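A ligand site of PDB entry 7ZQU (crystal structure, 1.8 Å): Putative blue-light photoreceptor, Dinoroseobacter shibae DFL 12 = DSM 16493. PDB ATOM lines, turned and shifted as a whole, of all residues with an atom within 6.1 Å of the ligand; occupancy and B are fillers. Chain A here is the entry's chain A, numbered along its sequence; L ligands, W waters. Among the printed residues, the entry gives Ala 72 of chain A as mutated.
ND2 of Asn 71 sits close to NH2 of Arg 89, at 3.2 Å. The side-chain hydroxyl (OG) of Ser 40 is in hydrogen-bond range of the side-chain amide oxygen (OD1) of Asn 47 (2.8 Å). N of Arg 73 is in hydrogen-bond range of OD1 of Asn 71, at 2.9 Å. ND2 of Asn 114 is in hydrogen-bond range of OD1 of Asn 104 (2.9 Å). The backbone carbonyl oxygen (O) of Arg 73 lies close to the side-chain amide oxygen (OE1) of Gln 76 (3.4 Å). N of Gly 133 is in hydrogen-bond range of O of Val 38 (2.9 Å). O of Leu 75 lies close to ND2 of Asn 104. OD1 of Asn 114 sits close to N of Leu 116, at 3.4 Å.
Val 38 touches the ligand (CG2 to C5, 3.6 Å). Ser 40 touches the ligand. Asn 47 touches the ligand. N of Ala 72 touches O3 of the ligand, at 3.5 Å. Leu 75 touches the ligand (CD1 to O2, 3.2 Å). CG1 of Val 85 touches O5 of the ligand (3.2 Å). Ile 88 touches the ligand (CG2 to C13, 3.5 Å). CD1 of Leu 92 touches O4 of the ligand (3.4 Å). Ile 102 touches the ligand (CD1 to O1, 3.7 Å). Leu 116 touches the ligand. O of Phe 131 touches C7 of the ligand (3.8 Å). Ala 132 touches the ligand. Gly 133 touches the ligand. Hydrophobic or aromatic side chains that line the ligand: Val 38, Ala 72, Leu 75, Val 85, Ile 88, Leu 92, Ile 102, Leu 116 and Phe 131. Of the 29 residues printed, 20 come within 4 Å of the ligand. The nearest printed residue that does not touch the ligand is Ile 118 (4.04 Å).
Water W1 lies within hydrogen-bond range of O9 of the ligand and OE1 of Gln 76. Water W2 lies within hydrogen-bond range of O of Asn 47 (3.0 Å), N of Ala 72 (3.1 Å), O3 of the ligand (3.1 Å) and ND2 of Asn 71 (3.5 Å).
The side-chain amide oxygen (OD1) of Asn 104 is in hydrogen-bond range of a nitrogen (N2) of the ligand, 2.9 Å away. O3 of the ligand is in hydrogen-bond range of OD1 of Asn 71 (2.6 Å). An oxygen (O2) of the ligand sits at hydrogen-bond distance from the side-chain amide nitrogen of Gln 135. The guanidinium group (NE) of Arg 73 lies within salt-bridge range of an oxygen (O9) of the ligand. NE2 of Gln 76 is in hydrogen-bond range of O5 of the ligand (2.8 Å). The guanidinium group of Arg 89 is in hydrogen-bond range of an oxygen (O4) of the ligand, 2.8 Å away. ND2 of Asn 114 sits at hydrogen-bond distance from O2 of the ligand (3.3 Å).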
ATOM      1  N   VAL A  38      16.632   6.487  -4.010  1.00  0.00           N
ATOM      2  CA  VAL A  38      17.224   6.264  -2.697  1.00  0.00           C
ATOM      3  C   VAL A  38      16.122   5.869  -1.730  1.00  0.00           C
ATOM      4  O   VAL A  38      14.949   6.187  -1.949  1.00  0.00           O
ATOM      5  CB  VAL A  38      18.006   7.479  -2.152  1.00  0.00           C
ATOM      6  CG1 VAL A  38      18.997   7.993  -3.194  1.00  0.00           C
ATOM      7  CG2 VAL A  38      17.086   8.589  -1.715  1.00  0.00           C
ATOM      8  N   PHE A  39      16.503   5.153  -0.686  1.00  0.00           N
ATOM      9  CA  PHE A  39      15.585   4.714   0.362  1.00  0.00           C
ATOM     10  C   PHE A  39      16.119   5.179   1.701  1.00  0.00           C
ATOM     11  O   PHE A  39      17.302   5.015   2.000  1.00  0.00           O
ATOM     12  CB  PHE A  39      15.428   3.186   0.355  1.00  0.00           C
ATOM     13  CG  PHE A  39      14.618   2.662  -0.805  1.00  0.00           C
ATOM     14  CD1 PHE A  39      15.145   2.670  -2.079  1.00  0.00           C
ATOM     15  CD2 PHE A  39      13.334   2.171  -0.620  1.00  0.00           C
ATOM     16  CE1 PHE A  39      14.412   2.208  -3.169  1.00  0.00           C
ATOM     17  CE2 PHE A  39      12.598   1.695  -1.715  1.00  0.00           C
ATOM     18  CZ  PHE A  39      13.148   1.714  -2.986  1.00  0.00           C
ATOM     19  N   SER A  40      15.248   5.751   2.526  1.00  0.00           N
ATOM     20  CA  SER A  40      15.644   6.258   3.834  1.00  0.00           C
ATOM     21  C   SER A  40      14.898   5.518   4.924  1.00  0.00           C
ATOM     22  O   SER A  40      13.818   4.955   4.703  1.00  0.00           O
ATOM     23  CB  SER A  40      15.390   7.757   3.948  1.00  0.00           C
ATOM     24  OG  SER A  40      14.002   7.970   4.182  1.00  0.00           O
ATOM     25  N   ASP A  46      17.991  11.380  11.996  1.00  0.00           N
ATOM     26  CA  ASP A  46      18.191  12.203  10.810  1.00  0.00           C
ATOM     27  C   ASP A  46      17.692  11.535   9.522  1.00  0.00           C
ATOM     28  O   ASP A  46      18.065  11.958   8.428  1.00  0.00           O
ATOM     29  CB  ASP A  46      19.660  12.630  10.647  1.00  0.00           C
ATOM     30  CG  ASP A  46      19.834  13.981   9.948  1.00  0.00           C
ATOM     31  OD1 ASP A  46      18.842  14.744   9.858  1.00  0.00           O
ATOM     32  OD2 ASP A  46      20.970  14.280   9.477  1.00  0.00           O
ATOM     33  N   ASN A  47      16.858  10.498   9.633  1.00  0.00           N
ATOM     34  CA  ASN A  47      16.235   9.864   8.474  1.00  0.00           C
ATOM     35  C   ASN A  47      17.256   9.523   7.382  1.00  0.00           C
ATOM     36  O   ASN A  47      17.145   9.994   6.246  1.00  0.00           O
ATOM     37  CB  ASN A  47      15.134  10.748   7.923  1.00  0.00           C
ATOM     38  CG  ASN A  47      14.311  10.065   6.868  1.00  0.00           C
ATOM     39  OD1 ASN A  47      14.226   8.846   6.817  1.00  0.00           O
ATOM     40  ND2 ASN A  47      13.696  10.863   6.005  1.00  0.00           N
ATOM     41  N   MET A  49      19.731   7.753   4.518  1.00  0.00           N
ATOM     42  CA  MET A  49      19.627   6.835   3.389  1.00  0.00           C
ATOM     43  C   MET A  49      20.266   5.500   3.749  1.00  0.00           C
ATOM     44  O   MET A  49      21.412   5.453   4.221  1.00  0.00           O
ATOM     45  CB  MET A  49      20.295   7.425   2.149  1.00  0.00           C
ATOM     46  CG  MET A  49      19.514   8.578   1.544  1.00  0.00           C
ATOM     47  SD  MET A  49      20.352   9.276   0.107  1.00  0.00           S
ATOM     48  CE  MET A  49      21.833   9.908   0.904  1.00  0.00           C
ATOM     49  N   PHE A  56      21.871   6.612  -8.930  1.00  0.00           N
ATOM     50  CA  PHE A  56      21.998   7.788  -8.061  1.00  0.00           C
ATOM     51  C   PHE A  56      23.463   8.173  -7.895  1.00  0.00           C
ATOM     52  O   PHE A  56      23.836   9.340  -8.038  1.00  0.00           O
ATOM     53  CB  PHE A  56      21.371   7.529  -6.700  1.00  0.00           C
ATOM     54  CG  PHE A  56      21.624   8.635  -5.681  1.00  0.00           C
ATOM     55  CD1 PHE A  56      20.809   9.742  -5.623  1.00  0.00           C
ATOM     56  CD2 PHE A  56      22.670   8.533  -4.790  1.00  0.00           C
ATOM     57  CE1 PHE A  56      21.049  10.749  -4.688  1.00  0.00           C
ATOM     58  CE2 PHE A  56      22.910   9.531  -3.850  1.00  0.00           C
ATOM     59  CZ  PHE A  56      22.093  10.633  -3.801  1.00  0.00           C
ATOM     60  N   ASN A  71      21.439  11.820   5.628  1.00  0.00           N
ATOM     61  CA  ASN A  71      20.238  12.435   5.083  1.00  0.00           C
ATOM     62  C   ASN A  71      20.504  13.005   3.707  1.00  0.00           C
ATOM     63  O   ASN A  71      21.585  13.551   3.438  1.00  0.00           O
ATOM     64  CB  ASN A  71      19.754  13.536   6.039  1.00  0.00           C
ATOM     65  CG  ASN A  71      18.418  14.105   5.642  1.00  0.00           C
ATOM     66  OD1 ASN A  71      18.316  14.904   4.724  1.00  0.00           O
ATOM     67  ND2 ASN A  71      17.360  13.690   6.362  1.00  0.00           N
ATOM     68  N   ALA A  72      19.523  12.876   2.797  1.00  0.00           N
ATOM     69  CA  ALA A  72      19.732  13.282   1.400  1.00  0.00           C
ATOM     70  C   ALA A  72      19.734  14.792   1.193  1.00  0.00           C
ATOM     71  O   ALA A  72      19.806  15.218   0.025  1.00  0.00           O
ATOM     72  CB  ALA A  72      18.648  12.644   0.515  1.00  0.00           C
ATOM     73  N   ARG A  73      19.664  15.625   2.235  1.00  0.00           N
ATOM     74  CA  ARG A  73      19.596  17.070   2.040  1.00  0.00           C
ATOM     75  C   ARG A  73      20.863  17.651   1.438  1.00  0.00           C
ATOM     76  O   ARG A  73      20.825  18.816   1.038  1.00  0.00           O
ATOM     77  CB  ARG A  73      19.303  17.787   3.360  1.00  0.00           C
ATOM     78  CG  ARG A  73      20.447  17.735   4.345  1.00  0.00           C
ATOM     79  CD  ARG A  73      20.235  18.660   5.558  1.00  0.00           C
ATOM     80  NE  ARG A  73      19.183  18.175   6.449  1.00  0.00           N
ATOM     81  CZ  ARG A  73      19.333  17.182   7.309  1.00  0.00           C
ATOM     82  NH1 ARG A  73      20.474  16.519   7.424  1.00  0.00           N
ATOM     83  NH2 ARG A  73      18.301  16.841   8.089  1.00  0.00           N
ATOM     84  N   LEU A  75      21.962  17.169  -1.364  1.00  0.00           N
ATOM     85  CA  LEU A  75      21.759  17.536  -2.760  1.00  0.00           C
ATOM     86  C   LEU A  75      21.350  18.995  -2.927  1.00  0.00           C
ATOM     87  O   LEU A  75      21.292  19.477  -4.055  1.00  0.00           O
ATOM     88  CB  LEU A  75      20.718  16.638  -3.420  1.00  0.00           C
ATOM     89  CG  LEU A  75      21.125  15.165  -3.563  1.00  0.00           C
ATOM     90  CD1 LEU A  75      20.101  14.424  -4.395  1.00  0.00           C
ATOM     91  CD2 LEU A  75      22.494  14.999  -4.168  1.00  0.00           C
ATOM     92  N   GLN A  76      21.083  19.695  -1.829  1.00  0.00           N
ATOM     93  CA  GLN A  76      20.781  21.113  -1.881  1.00  0.00           C
ATOM     94  C   GLN A  76      22.094  21.909  -1.930  1.00  0.00           C
ATOM     95  O   GLN A  76      23.181  21.369  -1.720  1.00  0.00           O
ATOM     96  CB  GLN A  76      19.920  21.505  -0.683  1.00  0.00           C
ATOM     97  CG  GLN A  76      18.569  20.785  -0.734  1.00  0.00           C
ATOM     98  CD  GLN A  76      17.996  20.472   0.644  1.00  0.00           C
ATOM     99  OE1 GLN A  76      18.367  21.082   1.644  1.00  0.00           O
ATOM    100  NE2 GLN A  76      17.074  19.501   0.692  1.00  0.00           N
ATOM    101  N   THR A  80      19.375  26.918  -3.603  1.00  0.00           N
ATOM    102  CA  THR A  80      18.148  26.182  -3.293  1.00  0.00           C
ATOM    103  C   THR A  80      17.232  27.033  -2.420  1.00  0.00           C
ATOM    104  O   THR A  80      17.691  27.758  -1.527  1.00  0.00           O
ATOM    105  CB  THR A  80      18.478  24.866  -2.584  1.00  0.00           C
ATOM    106  OG1 THR A  80      19.314  24.060  -3.409  1.00  0.00           O
ATOM    107  CG2 THR A  80      17.195  24.093  -2.268  1.00  0.00           C
ATOM    108  N   VAL A  85      12.858  23.198   0.868  1.00  0.00           N
ATOM    109  CA  VAL A  85      13.414  22.229   1.805  1.00  0.00           C
ATOM    110  C   VAL A  85      12.408  21.917   2.906  1.00  0.00           C
ATOM    111  O   VAL A  85      12.176  20.754   3.238  1.00  0.00           O
ATOM    112  CB  VAL A  85      14.738  22.763   2.384  1.00  0.00           C
ATOM    113  CG1 VAL A  85      15.283  21.797   3.412  1.00  0.00           C
ATOM    114  CG2 VAL A  85      15.732  23.009   1.262  1.00  0.00           C
ATOM    115  N   GLU A  86      11.817  22.959   3.491  1.00  0.00           N
ATOM    116  CA  GLU A  86      10.854  22.744   4.570  1.00  0.00           C
ATOM    117  C   GLU A  86       9.603  22.050   4.047  1.00  0.00           C
ATOM    118  O   GLU A  86       8.978  21.260   4.780  1.00  0.00           O
ATOM    119  CB  GLU A  86      10.527  24.065   5.240  1.00  0.00           C
ATOM    120  CG  GLU A  86       9.634  23.946   6.474  1.00  0.00           C
ATOM    121  CD  GLU A  86      10.229  23.110   7.609  1.00  0.00           C
ATOM    122  OE1 GLU A  86      11.471  22.964   7.650  1.00  0.00           O
ATOM    123  OE2 GLU A  86       9.445  22.612   8.460  1.00  0.00           O
ATOM    124  N   ILE A  88       9.542  19.670   1.836  1.00  0.00           N
ATOM    125  CA  ILE A  88       9.846  18.246   1.811  1.00  0.00           C
ATOM    126  C   ILE A  88       9.753  17.660   3.210  1.00  0.00           C
ATOM    127  O   ILE A  88       9.222  16.557   3.404  1.00  0.00           O
ATOM    128  CB  ILE A  88      11.244  17.998   1.208  1.00  0.00           C
ATOM    129  CG1 ILE A  88      11.295  18.476  -0.255  1.00  0.00           C
ATOM    130  CG2 ILE A  88      11.591  16.525   1.291  1.00  0.00           C
ATOM    131  CD1 ILE A  88      12.735  18.658  -0.764  1.00  0.00           C
ATOM    132  N   ARG A  89      10.263  18.389   4.205  1.00  0.00           N
ATOM    133  CA  ARG A  89      10.257  17.876   5.564  1.00  0.00           C
ATOM    134  C   ARG A  89       8.835  17.636   6.032  1.00  0.00           C
ATOM    135  O   ARG A  89       8.524  16.594   6.622  1.00  0.00           O
ATOM    136  CB  ARG A  89      11.009  18.848   6.485  1.00  0.00           C
ATOM    137  CG  ARG A  89      11.303  18.332   7.896  1.00  0.00           C
ATOM    138  CD  ARG A  89      11.563  16.826   7.965  1.00  0.00           C
ATOM    139  NE  ARG A  89      12.843  16.362   7.424  1.00  0.00           N
ATOM    140  CZ  ARG A  89      13.172  15.082   7.333  1.00  0.00           C
ATOM    141  NH1 ARG A  89      12.328  14.128   7.732  1.00  0.00           N
ATOM    142  NH2 ARG A  89      14.350  14.733   6.819  1.00  0.00           N
ATOM    143  N   LEU A  92       7.231  14.595   4.216  1.00  0.00           N
ATOM    144  CA  LEU A  92       7.646  13.347   4.853  1.00  0.00           C
ATOM    145  C   LEU A  92       6.859  13.087   6.140  1.00  0.00           C
ATOM    146  O   LEU A  92       6.400  11.965   6.376  1.00  0.00           O
ATOM    147  CB  LEU A  92       9.152  13.383   5.142  1.00  0.00           C
ATOM    148  CG  LEU A  92      10.052  13.411   3.908  1.00  0.00           C
ATOM    149  CD1 LEU A  92      11.501  13.738   4.309  1.00  0.00           C
ATOM    150  CD2 LEU A  92       9.977  12.106   3.151  1.00  0.00           C
ATOM    151  N   ILE A 102      12.861  21.212  -7.241  1.00  0.00           N
ATOM    152  CA  ILE A 102      13.811  21.812  -6.325  1.00  0.00           C
ATOM    153  C   ILE A 102      15.177  21.879  -7.002  1.00  0.00           C
ATOM    154  O   ILE A 102      15.568  20.946  -7.721  1.00  0.00           O
ATOM    155  CB  ILE A 102      13.847  21.043  -4.992  1.00  0.00           C
ATOM    156  CG1 ILE A 102      14.661  21.796  -3.936  1.00  0.00           C
ATOM    157  CG2 ILE A 102      14.294  19.600  -5.179  1.00  0.00           C
ATOM    158  CD1 ILE A 102      14.661  21.169  -2.555  1.00  0.00           C
ATOM    159  N   LEU A 103      15.859  23.003  -6.825  1.00  0.00           N
ATOM    160  CA  LEU A 103      17.209  23.156  -7.384  1.00  0.00           C
ATOM    161  C   LEU A 103      18.182  22.327  -6.555  1.00  0.00           C
ATOM    162  O   LEU A 103      18.252  22.474  -5.327  1.00  0.00           O
ATOM    163  CB  LEU A 103      17.612  24.634  -7.383  1.00  0.00           C
ATOM    164  CG  LEU A 103      18.945  24.956  -8.058  1.00  0.00           C
ATOM    165  CD1 LEU A 103      18.787  24.808  -9.565  1.00  0.00           C
ATOM    166  CD2 LEU A 103      19.400  26.346  -7.693  1.00  0.00           C
ATOM    167  N   ASN A 104      18.897  21.424  -7.220  1.00  0.00           N
ATOM    168  CA  ASN A 104      19.838  20.501  -6.577  1.00  0.00           C
ATOM    169  C   ASN A 104      21.199  20.610  -7.263  1.00  0.00           C
ATOM    170  O   ASN A 104      21.356  21.302  -8.273  1.00  0.00           O
ATOM    171  CB  ASN A 104      19.363  19.042  -6.620  1.00  0.00           C
ATOM    172  CG  ASN A 104      18.364  18.706  -5.520  1.00  0.00           C
ATOM    173  OD1 ASN A 104      17.854  17.584  -5.489  1.00  0.00           O
ATOM    174  ND2 ASN A 104      18.062  19.656  -4.644  1.00  0.00           N
ATOM    175  N   ASN A 114      15.639  19.394 -10.055  1.00  0.00           N
ATOM    176  CA  ASN A 114      15.224  18.037  -9.740  1.00  0.00           C
ATOM    177  C   ASN A 114      13.705  18.019  -9.561  1.00  0.00           C
ATOM    178  O   ASN A 114      13.184  18.734  -8.699  1.00  0.00           O
ATOM    179  CB  ASN A 114      15.917  17.568  -8.468  1.00  0.00           C
ATOM    180  CG  ASN A 114      15.626  16.130  -8.111  1.00  0.00           C
ATOM    181  OD1 ASN A 114      14.921  15.407  -8.827  1.00  0.00           O
ATOM    182  ND2 ASN A 114      16.180  15.702  -6.982  1.00  0.00           N
ATOM    183  N   LEU A 116      11.718  16.057  -7.878  1.00  0.00           N
ATOM    184  CA  LEU A 116      11.879  15.043  -6.862  1.00  0.00           C
ATOM    185  C   LEU A 116      10.533  14.396  -6.553  1.00  0.00           C
ATOM    186  O   LEU A 116       9.592  15.105  -6.239  1.00  0.00           O
ATOM    187  CB  LEU A 116      12.443  15.683  -5.593  1.00  0.00           C
ATOM    188  CG  LEU A 116      12.469  14.833  -4.330  1.00  0.00           C
ATOM    189  CD1 LEU A 116      13.356  13.614  -4.526  1.00  0.00           C
ATOM    190  CD2 LEU A 116      12.905  15.672  -3.117  1.00  0.00           C
ATOM    191  N   ILE A 118       8.661  11.587  -4.066  1.00  0.00           N
ATOM    192  CA  ILE A 118       8.830  10.824  -2.826  1.00  0.00           C
ATOM    193  C   ILE A 118       7.563  10.047  -2.556  1.00  0.00           C
ATOM    194  O   ILE A 118       6.456  10.573  -2.733  1.00  0.00           O
ATOM    195  CB  ILE A 118       9.175  11.756  -1.645  1.00  0.00           C
ATOM    196  CG1 ILE A 118      10.684  12.095  -1.690  1.00  0.00           C
ATOM    197  CG2 ILE A 118       8.838  11.074  -0.302  1.00  0.00           C
ATOM    198  CD1 ILE A 118      11.075  13.281  -0.837  1.00  0.00           C
ATOM    199  N   PHE A 131      10.948   5.523   3.256  1.00  0.00           N
ATOM    200  CA  PHE A 131      10.626   6.451   2.175  1.00  0.00           C
ATOM    201  C   PHE A 131      11.483   6.101   0.969  1.00  0.00           C
ATOM    202  O   PHE A 131      12.668   5.784   1.106  1.00  0.00           O
ATOM    203  CB  PHE A 131      10.869   7.892   2.574  1.00  0.00           C
ATOM    204  CG  PHE A 131       9.911   8.430   3.600  1.00  0.00           C
ATOM    205  CD1 PHE A 131       8.603   8.747   3.246  1.00  0.00           C
ATOM    206  CD2 PHE A 131      10.313   8.643   4.908  1.00  0.00           C
ATOM    207  CE1 PHE A 131       7.705   9.253   4.199  1.00  0.00           C
ATOM    208  CE2 PHE A 131       9.424   9.138   5.865  1.00  0.00           C
ATOM    209  CZ  PHE A 131       8.114   9.442   5.507  1.00  0.00           C
ATOM    210  N   ALA A 132      10.878   6.156  -0.212  1.00  0.00           N
ATOM    211  CA  ALA A 132      11.611   6.103  -1.479  1.00  0.00           C
ATOM    212  C   ALA A 132      11.601   7.481  -2.116  1.00  0.00           C
ATOM    213  O   ALA A 132      10.567   8.167  -2.102  1.00  0.00           O
ATOM    214  CB  ALA A 132      11.000   5.077  -2.432  1.00  0.00           C
ATOM    215  N   GLY A 133      12.742   7.919  -2.646  1.00  0.00           N
ATOM    216  CA  GLY A 133      12.765   9.201  -3.331  1.00  0.00           C
ATOM    217  C   GLY A 133      13.472   9.092  -4.667  1.00  0.00           C
ATOM    218  O   GLY A 133      14.581   8.526  -4.719  1.00  0.00           O
ATOM    219  N   ALA A 134      12.873   9.595  -5.747  1.00  0.00           N
ATOM    220  CA  ALA A 134      13.471   9.498  -7.081  1.00  0.00           C
ATOM    221  C   ALA A 134      13.908  10.862  -7.595  1.00  0.00           C
ATOM    222  O   ALA A 134      13.133  11.836  -7.545  1.00  0.00           O
ATOM    223  CB  ALA A 134      12.495   8.842  -8.067  1.00  0.00           C
ATOM    224  N   GLN A 135      15.130  10.949  -8.110  1.00  0.00           N
ATOM    225  CA  GLN A 135      15.684  12.174  -8.676  1.00  0.00           C
ATOM    226  C   GLN A 135      15.435  12.170 -10.184  1.00  0.00           C
ATOM    227  O   GLN A 135      15.689  11.172 -10.857  1.00  0.00           O
ATOM    228  CB  GLN A 135      17.181  12.288  -8.391  1.00  0.00           C
ATOM    229  CG  GLN A 135      17.554  12.386  -6.895  1.00  0.00           C
ATOM    230  CD  GLN A 135      17.238  11.108  -6.105  1.00  0.00           C
ATOM    231  OE1 GLN A 135      17.431   9.991  -6.584  1.00  0.00           O
ATOM    232  NE2 GLN A 135      16.753  11.291  -4.890  1.00  0.00           N
HETATM  233  N1  LIG L   1      16.112  16.632  -0.845  1.00  0.00           N
HETATM  234  C1  LIG L   1      16.659  17.147  -1.969  1.00  0.00           C
HETATM  235  O1  LIG L   1      16.940  18.343  -2.054  1.00  0.00           O
HETATM  236  N2  LIG L   1      16.934  16.369  -3.063  1.00  0.00           N
HETATM  237  C2  LIG L   1      16.652  15.022  -3.072  1.00  0.00           C
HETATM  238  O2  LIG L   1      16.894  14.372  -4.078  1.00  0.00           O
HETATM  239  C3  LIG L   1      16.070  14.450  -1.913  1.00  0.00           C
HETATM  240  N3  LIG L   1      15.797  13.161  -1.918  1.00  0.00           N
HETATM  241  C4  LIG L   1      15.221  12.646  -0.777  1.00  0.00           C
HETATM  242  C5  LIG L   1      14.908  11.273  -0.756  1.00  0.00           C
HETATM  243  C6  LIG L   1      14.307  10.688   0.333  1.00  0.00           C
HETATM  244  C7  LIG L   1      13.977   9.218   0.339  1.00  0.00           C
HETATM  245  C8  LIG L   1      14.037  11.471   1.481  1.00  0.00           C
HETATM  246  C9  LIG L   1      13.412  10.843   2.698  1.00  0.00           C
HETATM  247  C10 LIG L   1      14.350  12.822   1.482  1.00  0.00           C
HETATM  248  C11 LIG L   1      14.941  13.435   0.357  1.00  0.00           C
HETATM  249  N4  LIG L   1      15.261  14.788   0.322  1.00  0.00           N
HETATM  250  C12 LIG L   1      15.823  15.351  -0.817  1.00  0.00           C
HETATM  251  C13 LIG L   1      14.934  15.666   1.466  1.00  0.00           C
HETATM  252  C14 LIG L   1      15.989  15.760   2.562  1.00  0.00           C
HETATM  253  O3  LIG L   1      16.387  14.470   2.986  1.00  0.00           O
HETATM  254  C15 LIG L   1      15.392  16.493   3.768  1.00  0.00           C
HETATM  255  O4  LIG L   1      14.247  15.770   4.273  1.00  0.00           O
HETATM  256  C16 LIG L   1      14.972  17.938   3.508  1.00  0.00           C
HETATM  257  O5  LIG L   1      16.119  18.736   3.214  1.00  0.00           O
HETATM  258  C17 LIG L   1      14.199  18.537   4.665  1.00  0.00           C
HETATM  259  O6  LIG L   1      14.822  18.265   5.953  1.00  0.00           O
HETATM  260  P1  LIG L   1      15.926  19.279   6.566  1.00  0.00           P
HETATM  261  O7  LIG L   1      15.246  20.634   6.691  1.00  0.00           O
HETATM  262  O8  LIG L   1      16.306  18.700   7.914  1.00  0.00           O
HETATM  263  O9  LIG L   1      17.094  19.303   5.593  1.00  0.00           O
HETATM  264  O   HOH W   1      18.688  21.701   4.631  1.00  0.00           O
HETATM  265  O   HOH W   2      16.959  11.496   3.707  1.00  0.00           O
